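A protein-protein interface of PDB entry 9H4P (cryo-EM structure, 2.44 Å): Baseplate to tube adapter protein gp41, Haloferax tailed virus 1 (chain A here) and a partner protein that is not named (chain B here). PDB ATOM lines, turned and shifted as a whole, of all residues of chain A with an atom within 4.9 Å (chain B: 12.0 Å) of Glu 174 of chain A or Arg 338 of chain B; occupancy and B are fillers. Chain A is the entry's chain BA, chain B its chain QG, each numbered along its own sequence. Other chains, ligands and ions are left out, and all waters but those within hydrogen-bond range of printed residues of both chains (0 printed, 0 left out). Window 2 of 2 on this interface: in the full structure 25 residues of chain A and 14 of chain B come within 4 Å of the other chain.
The side-chain carboxylate (OE1) of Glu 174 of chain A is in salt-bridge range of the guanidinium group (NH1) of Arg 338 of chain B (2.8 Å). OG of Ser 336 of chain B sits at hydrogen-bond distance from OG1 of Thr 111 of chain A (3.2 Å). OG of Ser 336 of chain B sits at hydrogen-bond distance from O of Ser 125 of chain A, at 2.7 Å.
Thr 111 of chain A touches Arg 338 of chain B (CG2 to CB, 3.97 Å). Glu 113 of chain A touches Arg 338 of chain B (OE2 to C, 3.1 Å). Ser 125 of chain A touches Arg 337 of chain B (CB to N, 3.98 Å).
Of the 12 printed residues of chain A, 4 touch a printed residue of chain B. Printed residues of chain A that touch a printed residue of chain B: Thr 111, Glu 113, Ser 125 and Glu 174.
The backbone carbonyl oxygen (O) of Ser 125 of chain A sits at hydrogen-bond distance from the backbone NH (N) of Thr 111 of chain A (2.8 Å). The backbone carbonyl oxygen of Glu 174 of chain A lies within hydrogen-bond range of the backbone NH of Thr 207 of chain A (2.7 Å). O of Pro 335 of chain B lies within hydrogen-bond range of NH1 of Arg 337 of chain B.
Of chain B, only Arg 338 comes within 4 Å of Glu 174 of chain A. Of chain A, only Thr 111 (3.97 Å), Glu 113 (3.1 Å) and Glu 174 (2.8 Å) come within 4 Å of Arg 338 of chain B. Thr 111 of chain A touches just these residues of chain B: Ser 336 and Arg 338. Of chain B, only Arg 338 (3.1 Å) comes within 4 Å of Glu 113 of chain A. Ser 125 of chain A touches just these residues of chain B: Ser 336 (2.7 Å) and Arg 337 (3.98 Å). No residue of chain B comes within 4 Å of Ser 172 of chain A. No residue of chain B comes within 4 Å of Val 173 of chain A. No residue of chain B comes within 4 Å of Thr 176 of chain A. No residue of chain B comes within 4 Å of Val 205 of chain A. No residue of chain B comes within 4 Å of Phe 206 of chain A. No residue of chain B comes within 4 Å of Thr 207 of chain A. Of the printed residues of chain A, Arg 337 of chain B touches Ser 125 (3.98 Å). Of the printed residues of chain A, Ser 336 of chain B touches Thr 111 and Ser 125. The nearest printed residue of chain A that does not touch Arg 337 of chain B is Thr 111 of chain A (5.5 Å).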
ATOM      1  N   THR A 111     -10.376  10.664  -2.529  1.00  0.00           N
ATOM      2  CA  THR A 111     -10.027  11.781  -1.660  1.00  0.00           C
ATOM      3  C   THR A 111     -11.131  11.974  -0.621  1.00  0.00           C
ATOM      4  O   THR A 111     -12.320  11.972  -0.954  1.00  0.00           O
ATOM      5  CB  THR A 111      -9.795  13.080  -2.450  1.00  0.00           C
ATOM      6  OG1 THR A 111      -8.685  12.882  -3.326  1.00  0.00           O
ATOM      7  CG2 THR A 111      -9.537  14.299  -1.587  1.00  0.00           C
ATOM      8  N   LEU A 112     -10.705  12.147   0.638  1.00  0.00           N
ATOM      9  CA  LEU A 112     -11.568  12.492   1.760  1.00  0.00           C
ATOM     10  C   LEU A 112     -11.119  13.848   2.307  1.00  0.00           C
ATOM     11  O   LEU A 112      -9.941  14.021   2.624  1.00  0.00           O
ATOM     12  CB  LEU A 112     -11.439  11.400   2.833  1.00  0.00           C
ATOM     13  CG  LEU A 112     -11.857   9.981   2.421  1.00  0.00           C
ATOM     14  CD1 LEU A 112     -11.400   8.942   3.445  1.00  0.00           C
ATOM     15  CD2 LEU A 112     -13.365   9.876   2.200  1.00  0.00           C
ATOM     16  N   GLU A 113     -12.056  14.803   2.406  1.00  0.00           N
ATOM     17  CA  GLU A 113     -11.739  16.104   2.982  1.00  0.00           C
ATOM     18  C   GLU A 113     -12.538  16.316   4.268  1.00  0.00           C
ATOM     19  O   GLU A 113     -13.761  16.152   4.289  1.00  0.00           O
ATOM     20  CB  GLU A 113     -11.973  17.249   1.989  1.00  0.00           C
ATOM     21  CG  GLU A 113     -11.294  17.055   0.648  1.00  0.00           C
ATOM     22  CD  GLU A 113     -11.400  18.244  -0.283  1.00  0.00           C
ATOM     23  OE1 GLU A 113     -11.274  19.388   0.189  1.00  0.00           O
ATOM     24  OE2 GLU A 113     -11.607  18.017  -1.474  1.00  0.00           O
ATOM     25  N   SER A 125     -14.591  12.398  -2.803  1.00  0.00           N
ATOM     26  CA  SER A 125     -14.455  12.283  -4.246  1.00  0.00           C
ATOM     27  C   SER A 125     -13.800  10.943  -4.589  1.00  0.00           C
ATOM     28  O   SER A 125     -12.678  10.671  -4.153  1.00  0.00           O
ATOM     29  CB  SER A 125     -13.704  13.455  -4.832  1.00  0.00           C
ATOM     30  OG  SER A 125     -14.527  14.612  -4.866  1.00  0.00           O
ATOM     31  N   SER A 172      -7.476  21.934   8.689  1.00  0.00           N
ATOM     32  CA  SER A 172      -8.187  21.087   7.737  1.00  0.00           C
ATOM     33  C   SER A 172      -7.316  19.890   7.353  1.00  0.00           C
ATOM     34  O   SER A 172      -6.097  20.032   7.219  1.00  0.00           O
ATOM     35  CB  SER A 172      -8.583  21.863   6.503  1.00  0.00           C
ATOM     36  OG  SER A 172      -9.409  22.964   6.840  1.00  0.00           O
ATOM     37  N   VAL A 173      -7.951  18.722   7.154  1.00  0.00           N
ATOM     38  CA  VAL A 173      -7.266  17.509   6.707  1.00  0.00           C
ATOM     39  C   VAL A 173      -7.854  17.063   5.368  1.00  0.00           C
ATOM     40  O   VAL A 173      -9.072  16.953   5.224  1.00  0.00           O
ATOM     41  CB  VAL A 173      -7.324  16.365   7.752  1.00  0.00           C
ATOM     42  CG1 VAL A 173      -6.869  15.012   7.202  1.00  0.00           C
ATOM     43  CG2 VAL A 173      -6.531  16.694   9.009  1.00  0.00           C
ATOM     44  N   GLU A 174      -6.966  16.800   4.401  1.00  0.00           N
ATOM     45  CA  GLU A 174      -7.299  16.051   3.198  1.00  0.00           C
ATOM     46  C   GLU A 174      -6.500  14.746   3.216  1.00  0.00           C
ATOM     47  O   GLU A 174      -5.273  14.780   3.337  1.00  0.00           O
ATOM     48  CB  GLU A 174      -6.992  16.918   1.970  1.00  0.00           C
ATOM     49  CG  GLU A 174      -7.118  16.215   0.625  1.00  0.00           C
ATOM     50  CD  GLU A 174      -6.685  17.045  -0.570  1.00  0.00           C
ATOM     51  OE1 GLU A 174      -6.403  18.243  -0.395  1.00  0.00           O
ATOM     52  OE2 GLU A 174      -6.632  16.488  -1.676  1.00  0.00           O
ATOM     53  N   ARG A 175      -7.195  13.604   3.110  1.00  0.00           N
ATOM     54  CA  ARG A 175      -6.528  12.319   2.929  1.00  0.00           C
ATOM     55  C   ARG A 175      -6.809  11.809   1.511  1.00  0.00           C
ATOM     56  O   ARG A 175      -7.960  11.828   1.074  1.00  0.00           O
ATOM     57  CB  ARG A 175      -6.936  11.327   4.029  1.00  0.00           C
ATOM     58  CG  ARG A 175      -6.094  10.057   4.056  1.00  0.00           C
ATOM     59  CD  ARG A 175      -6.810   8.939   4.790  1.00  0.00           C
ATOM     60  NE  ARG A 175      -6.040   7.702   4.759  1.00  0.00           N
ATOM     61  CZ  ARG A 175      -6.350   6.579   5.404  1.00  0.00           C
ATOM     62  NH1 ARG A 175      -5.564   5.522   5.291  1.00  0.00           N
ATOM     63  NH2 ARG A 175      -7.435   6.504   6.160  1.00  0.00           N
ATOM     64  N   THR A 176      -5.759  11.378   0.788  1.00  0.00           N
ATOM     65  CA  THR A 176      -5.950  10.747  -0.516  1.00  0.00           C
ATOM     66  C   THR A 176      -5.361   9.335  -0.527  1.00  0.00           C
ATOM     67  O   THR A 176      -4.360   9.063   0.141  1.00  0.00           O
ATOM     68  CB  THR A 176      -5.470  11.603  -1.703  1.00  0.00           C
ATOM     69  OG1 THR A 176      -4.085  11.384  -1.981  1.00  0.00           O
ATOM     70  CG2 THR A 176      -5.747  13.085  -1.572  1.00  0.00           C
ATOM     71  N   VAL A 205      -1.858   9.366   1.564  1.00  0.00           N
ATOM     72  CA  VAL A 205      -1.266  10.673   1.830  1.00  0.00           C
ATOM     73  C   VAL A 205      -2.203  11.470   2.738  1.00  0.00           C
ATOM     74  O   VAL A 205      -3.414  11.504   2.510  1.00  0.00           O
ATOM     75  CB  VAL A 205      -0.965  11.440   0.518  1.00  0.00           C
ATOM     76  CG1 VAL A 205      -0.600  12.907   0.740  1.00  0.00           C
ATOM     77  CG2 VAL A 205       0.099  10.760  -0.340  1.00  0.00           C
ATOM     78  N   PHE A 206      -1.615  12.120   3.752  1.00  0.00           N
ATOM     79  CA  PHE A 206      -2.317  13.073   4.599  1.00  0.00           C
ATOM     80  C   PHE A 206      -1.768  14.471   4.327  1.00  0.00           C
ATOM     81  O   PHE A 206      -0.558  14.696   4.413  1.00  0.00           O
ATOM     82  CB  PHE A 206      -2.147  12.706   6.076  1.00  0.00           C
ATOM     83  CG  PHE A 206      -2.801  11.414   6.495  1.00  0.00           C
ATOM     84  CD1 PHE A 206      -4.123  11.406   6.925  1.00  0.00           C
ATOM     85  CD2 PHE A 206      -2.098  10.214   6.474  1.00  0.00           C
ATOM     86  CE1 PHE A 206      -4.727  10.225   7.333  1.00  0.00           C
ATOM     87  CE2 PHE A 206      -2.707   9.029   6.873  1.00  0.00           C
ATOM     88  CZ  PHE A 206      -4.021   9.038   7.299  1.00  0.00           C
ATOM     89  N   THR A 207      -2.677  15.395   3.985  1.00  0.00           N
ATOM     90  CA  THR A 207      -2.351  16.802   3.811  1.00  0.00           C
ATOM     91  C   THR A 207      -3.047  17.613   4.901  1.00  0.00           C
ATOM     92  O   THR A 207      -4.271  17.550   5.039  1.00  0.00           O
ATOM     93  CB  THR A 207      -2.809  17.326   2.441  1.00  0.00           C
ATOM     94  OG1 THR A 207      -2.297  16.478   1.412  1.00  0.00           O
ATOM     95  CG2 THR A 207      -2.388  18.755   2.169  1.00  0.00           C
ATOM     96  N   GLY B 292     -18.217  30.031  -4.638  1.00  0.00           N
ATOM     97  CA  GLY B 292     -18.036  28.615  -4.344  1.00  0.00           C
ATOM     98  C   GLY B 292     -18.616  27.689  -5.410  1.00  0.00           C
ATOM     99  O   GLY B 292     -19.712  27.928  -5.905  1.00  0.00           O
ATOM    100  N   GLY B 293     -17.867  26.630  -5.740  1.00  0.00           N
ATOM    101  CA  GLY B 293     -18.311  25.583  -6.647  1.00  0.00           C
ATOM    102  C   GLY B 293     -18.604  26.098  -8.053  1.00  0.00           C
ATOM    103  O   GLY B 293     -17.704  26.587  -8.731  1.00  0.00           O
ATOM    104  N   GLY B 300     -13.958  29.482 -13.262  1.00  0.00           N
ATOM    105  CA  GLY B 300     -13.728  28.166 -12.683  1.00  0.00           C
ATOM    106  C   GLY B 300     -13.835  27.033 -13.700  1.00  0.00           C
ATOM    107  O   GLY B 300     -12.824  26.416 -14.024  1.00  0.00           O
ATOM    108  N   ASN B 301     -15.054  26.771 -14.197  1.00  0.00           N
ATOM    109  CA  ASN B 301     -15.353  25.621 -15.045  1.00  0.00           C
ATOM    110  C   ASN B 301     -14.539  25.669 -16.339  1.00  0.00           C
ATOM    111  O   ASN B 301     -14.039  24.640 -16.793  1.00  0.00           O
ATOM    112  CB  ASN B 301     -16.855  25.472 -15.305  1.00  0.00           C
ATOM    113  CG  ASN B 301     -17.683  25.222 -14.061  1.00  0.00           C
ATOM    114  OD1 ASN B 301     -17.165  24.822 -13.023  1.00  0.00           O
ATOM    115  ND2 ASN B 301     -18.980  25.448 -14.162  1.00  0.00           N
ATOM    116  N   ARG B 304     -11.109  24.443 -15.142  1.00  0.00           N
ATOM    117  CA  ARG B 304     -11.096  23.086 -14.605  1.00  0.00           C
ATOM    118  C   ARG B 304     -11.048  22.065 -15.745  1.00  0.00           C
ATOM    119  O   ARG B 304     -10.373  21.044 -15.627  1.00  0.00           O
ATOM    120  CB  ARG B 304     -12.312  22.859 -13.695  1.00  0.00           C
ATOM    121  CG  ARG B 304     -12.275  23.585 -12.357  1.00  0.00           C
ATOM    122  CD  ARG B 304     -13.653  23.828 -11.761  1.00  0.00           C
ATOM    123  NE  ARG B 304     -13.600  24.608 -10.527  1.00  0.00           N
ATOM    124  CZ  ARG B 304     -14.586  25.332  -9.998  1.00  0.00           C
ATOM    125  NH1 ARG B 304     -14.379  25.985  -8.868  1.00  0.00           N
ATOM    126  NH2 ARG B 304     -15.764  25.412 -10.585  1.00  0.00           N
ATOM    127  N   PHE B 307      -7.536  22.216 -17.581  1.00  0.00           N
ATOM    128  CA  PHE B 307      -6.603  21.591 -16.651  1.00  0.00           C
ATOM    129  C   PHE B 307      -6.562  20.077 -16.860  1.00  0.00           C
ATOM    130  O   PHE B 307      -5.475  19.510 -16.919  1.00  0.00           O
ATOM    131  CB  PHE B 307      -6.880  21.978 -15.194  1.00  0.00           C
ATOM    132  CG  PHE B 307      -5.988  23.060 -14.637  1.00  0.00           C
ATOM    133  CD1 PHE B 307      -4.624  22.854 -14.507  1.00  0.00           C
ATOM    134  CD2 PHE B 307      -6.511  24.280 -14.231  1.00  0.00           C
ATOM    135  CE1 PHE B 307      -3.801  23.847 -14.001  1.00  0.00           C
ATOM    136  CE2 PHE B 307      -5.689  25.271 -13.719  1.00  0.00           C
ATOM    137  CZ  PHE B 307      -4.336  25.051 -13.606  1.00  0.00           C
ATOM    138  N   ALA B 308      -7.734  19.437 -16.984  1.00  0.00           N
ATOM    139  CA  ALA B 308      -7.826  18.016 -17.288  1.00  0.00           C
ATOM    140  C   ALA B 308      -7.304  17.711 -18.693  1.00  0.00           C
ATOM    141  O   ALA B 308      -6.584  16.735 -18.875  1.00  0.00           O
ATOM    142  CB  ALA B 308      -9.240  17.532 -17.097  1.00  0.00           C
ATOM    143  N   PHE B 311      -3.503  17.952 -18.705  1.00  0.00           N
ATOM    144  CA  PHE B 311      -2.936  16.872 -17.905  1.00  0.00           C
ATOM    145  C   PHE B 311      -2.919  15.555 -18.685  1.00  0.00           C
ATOM    146  O   PHE B 311      -1.993  14.766 -18.515  1.00  0.00           O
ATOM    147  CB  PHE B 311      -3.641  16.763 -16.548  1.00  0.00           C
ATOM    148  CG  PHE B 311      -3.165  15.669 -15.622  1.00  0.00           C
ATOM    149  CD1 PHE B 311      -1.818  15.496 -15.349  1.00  0.00           C
ATOM    150  CD2 PHE B 311      -4.073  14.833 -14.989  1.00  0.00           C
ATOM    151  CE1 PHE B 311      -1.391  14.494 -14.492  1.00  0.00           C
ATOM    152  CE2 PHE B 311      -3.645  13.834 -14.128  1.00  0.00           C
ATOM    153  CZ  PHE B 311      -2.304  13.667 -13.883  1.00  0.00           C
ATOM    154  N   ASP B 334      -8.989   9.444 -15.067  1.00  0.00           N
ATOM    155  CA  ASP B 334      -8.680  10.700 -14.390  1.00  0.00           C
ATOM    156  C   ASP B 334      -8.790  10.582 -12.866  1.00  0.00           C
ATOM    157  O   ASP B 334      -9.644   9.850 -12.362  1.00  0.00           O
ATOM    158  CB  ASP B 334      -9.496  11.866 -14.958  1.00  0.00           C
ATOM    159  CG  ASP B 334      -9.030  12.332 -16.325  1.00  0.00           C
ATOM    160  OD1 ASP B 334      -7.868  12.066 -16.676  1.00  0.00           O
ATOM    161  OD2 ASP B 334      -9.834  12.966 -17.022  1.00  0.00           O
ATOM    162  N   PRO B 335      -7.929  11.302 -12.093  1.00  0.00           N
ATOM    163  CA  PRO B 335      -7.918  11.216 -10.630  1.00  0.00           C
ATOM    164  C   PRO B 335      -9.076  11.961  -9.968  1.00  0.00           C
ATOM    165  O   PRO B 335      -9.794  12.715 -10.623  1.00  0.00           O
ATOM    166  CB  PRO B 335      -6.579  11.870 -10.247  1.00  0.00           C
ATOM    167  CG  PRO B 335      -6.340  12.886 -11.337  1.00  0.00           C
ATOM    168  CD  PRO B 335      -6.898  12.237 -12.586  1.00  0.00           C
ATOM    169  N   SER B 336      -9.216  11.737  -8.654  1.00  0.00           N
ATOM    170  CA  SER B 336     -10.214  12.353  -7.790  1.00  0.00           C
ATOM    171  C   SER B 336     -10.148  13.884  -7.857  1.00  0.00           C
ATOM    172  O   SER B 336      -9.057  14.446  -7.902  1.00  0.00           O
ATOM    173  CB  SER B 336     -10.022  11.842  -6.383  1.00  0.00           C
ATOM    174  OG  SER B 336     -11.012  12.342  -5.507  1.00  0.00           O
ATOM    175  N   ARG B 337     -11.321  14.540  -7.823  1.00  0.00           N
ATOM    176  CA  ARG B 337     -11.519  15.961  -8.107  1.00  0.00           C
ATOM    177  C   ARG B 337     -10.923  16.881  -7.035  1.00  0.00           C
ATOM    178  O   ARG B 337     -10.558  18.011  -7.349  1.00  0.00           O
ATOM    179  CB  ARG B 337     -13.006  16.281  -8.305  1.00  0.00           C
ATOM    180  CG  ARG B 337     -13.684  15.581  -9.478  1.00  0.00           C
ATOM    181  CD  ARG B 337     -13.218  15.993 -10.862  1.00  0.00           C
ATOM    182  NE  ARG B 337     -11.976  15.318 -11.207  1.00  0.00           N
ATOM    183  CZ  ARG B 337     -11.046  15.775 -12.037  1.00  0.00           C
ATOM    184  NH1 ARG B 337      -9.960  15.058 -12.250  1.00  0.00           N
ATOM    185  NH2 ARG B 337     -11.189  16.937 -12.646  1.00  0.00           N
ATOM    186  N   ARG B 338     -10.857  16.402  -5.780  1.00  0.00           N
ATOM    187  CA  ARG B 338     -10.350  17.093  -4.593  1.00  0.00           C
ATOM    188  C   ARG B 338     -10.960  18.494  -4.434  1.00  0.00           C
ATOM    189  O   ARG B 338     -10.381  19.521  -4.760  1.00  0.00           O
ATOM    190  CB  ARG B 338      -8.826  16.979  -4.422  1.00  0.00           C
ATOM    191  CG  ARG B 338      -7.950  17.605  -5.501  1.00  0.00           C
ATOM    192  CD  ARG B 338      -6.462  17.495  -5.214  1.00  0.00           C
ATOM    193  NE  ARG B 338      -6.146  18.108  -3.934  1.00  0.00           N
ATOM    194  CZ  ARG B 338      -5.692  19.341  -3.758  1.00  0.00           C
ATOM    195  NH1 ARG B 338      -5.471  19.780  -2.534  1.00  0.00           N
ATOM    196  NH2 ARG B 338      -5.454  20.130  -4.788  1.00  0.00           N
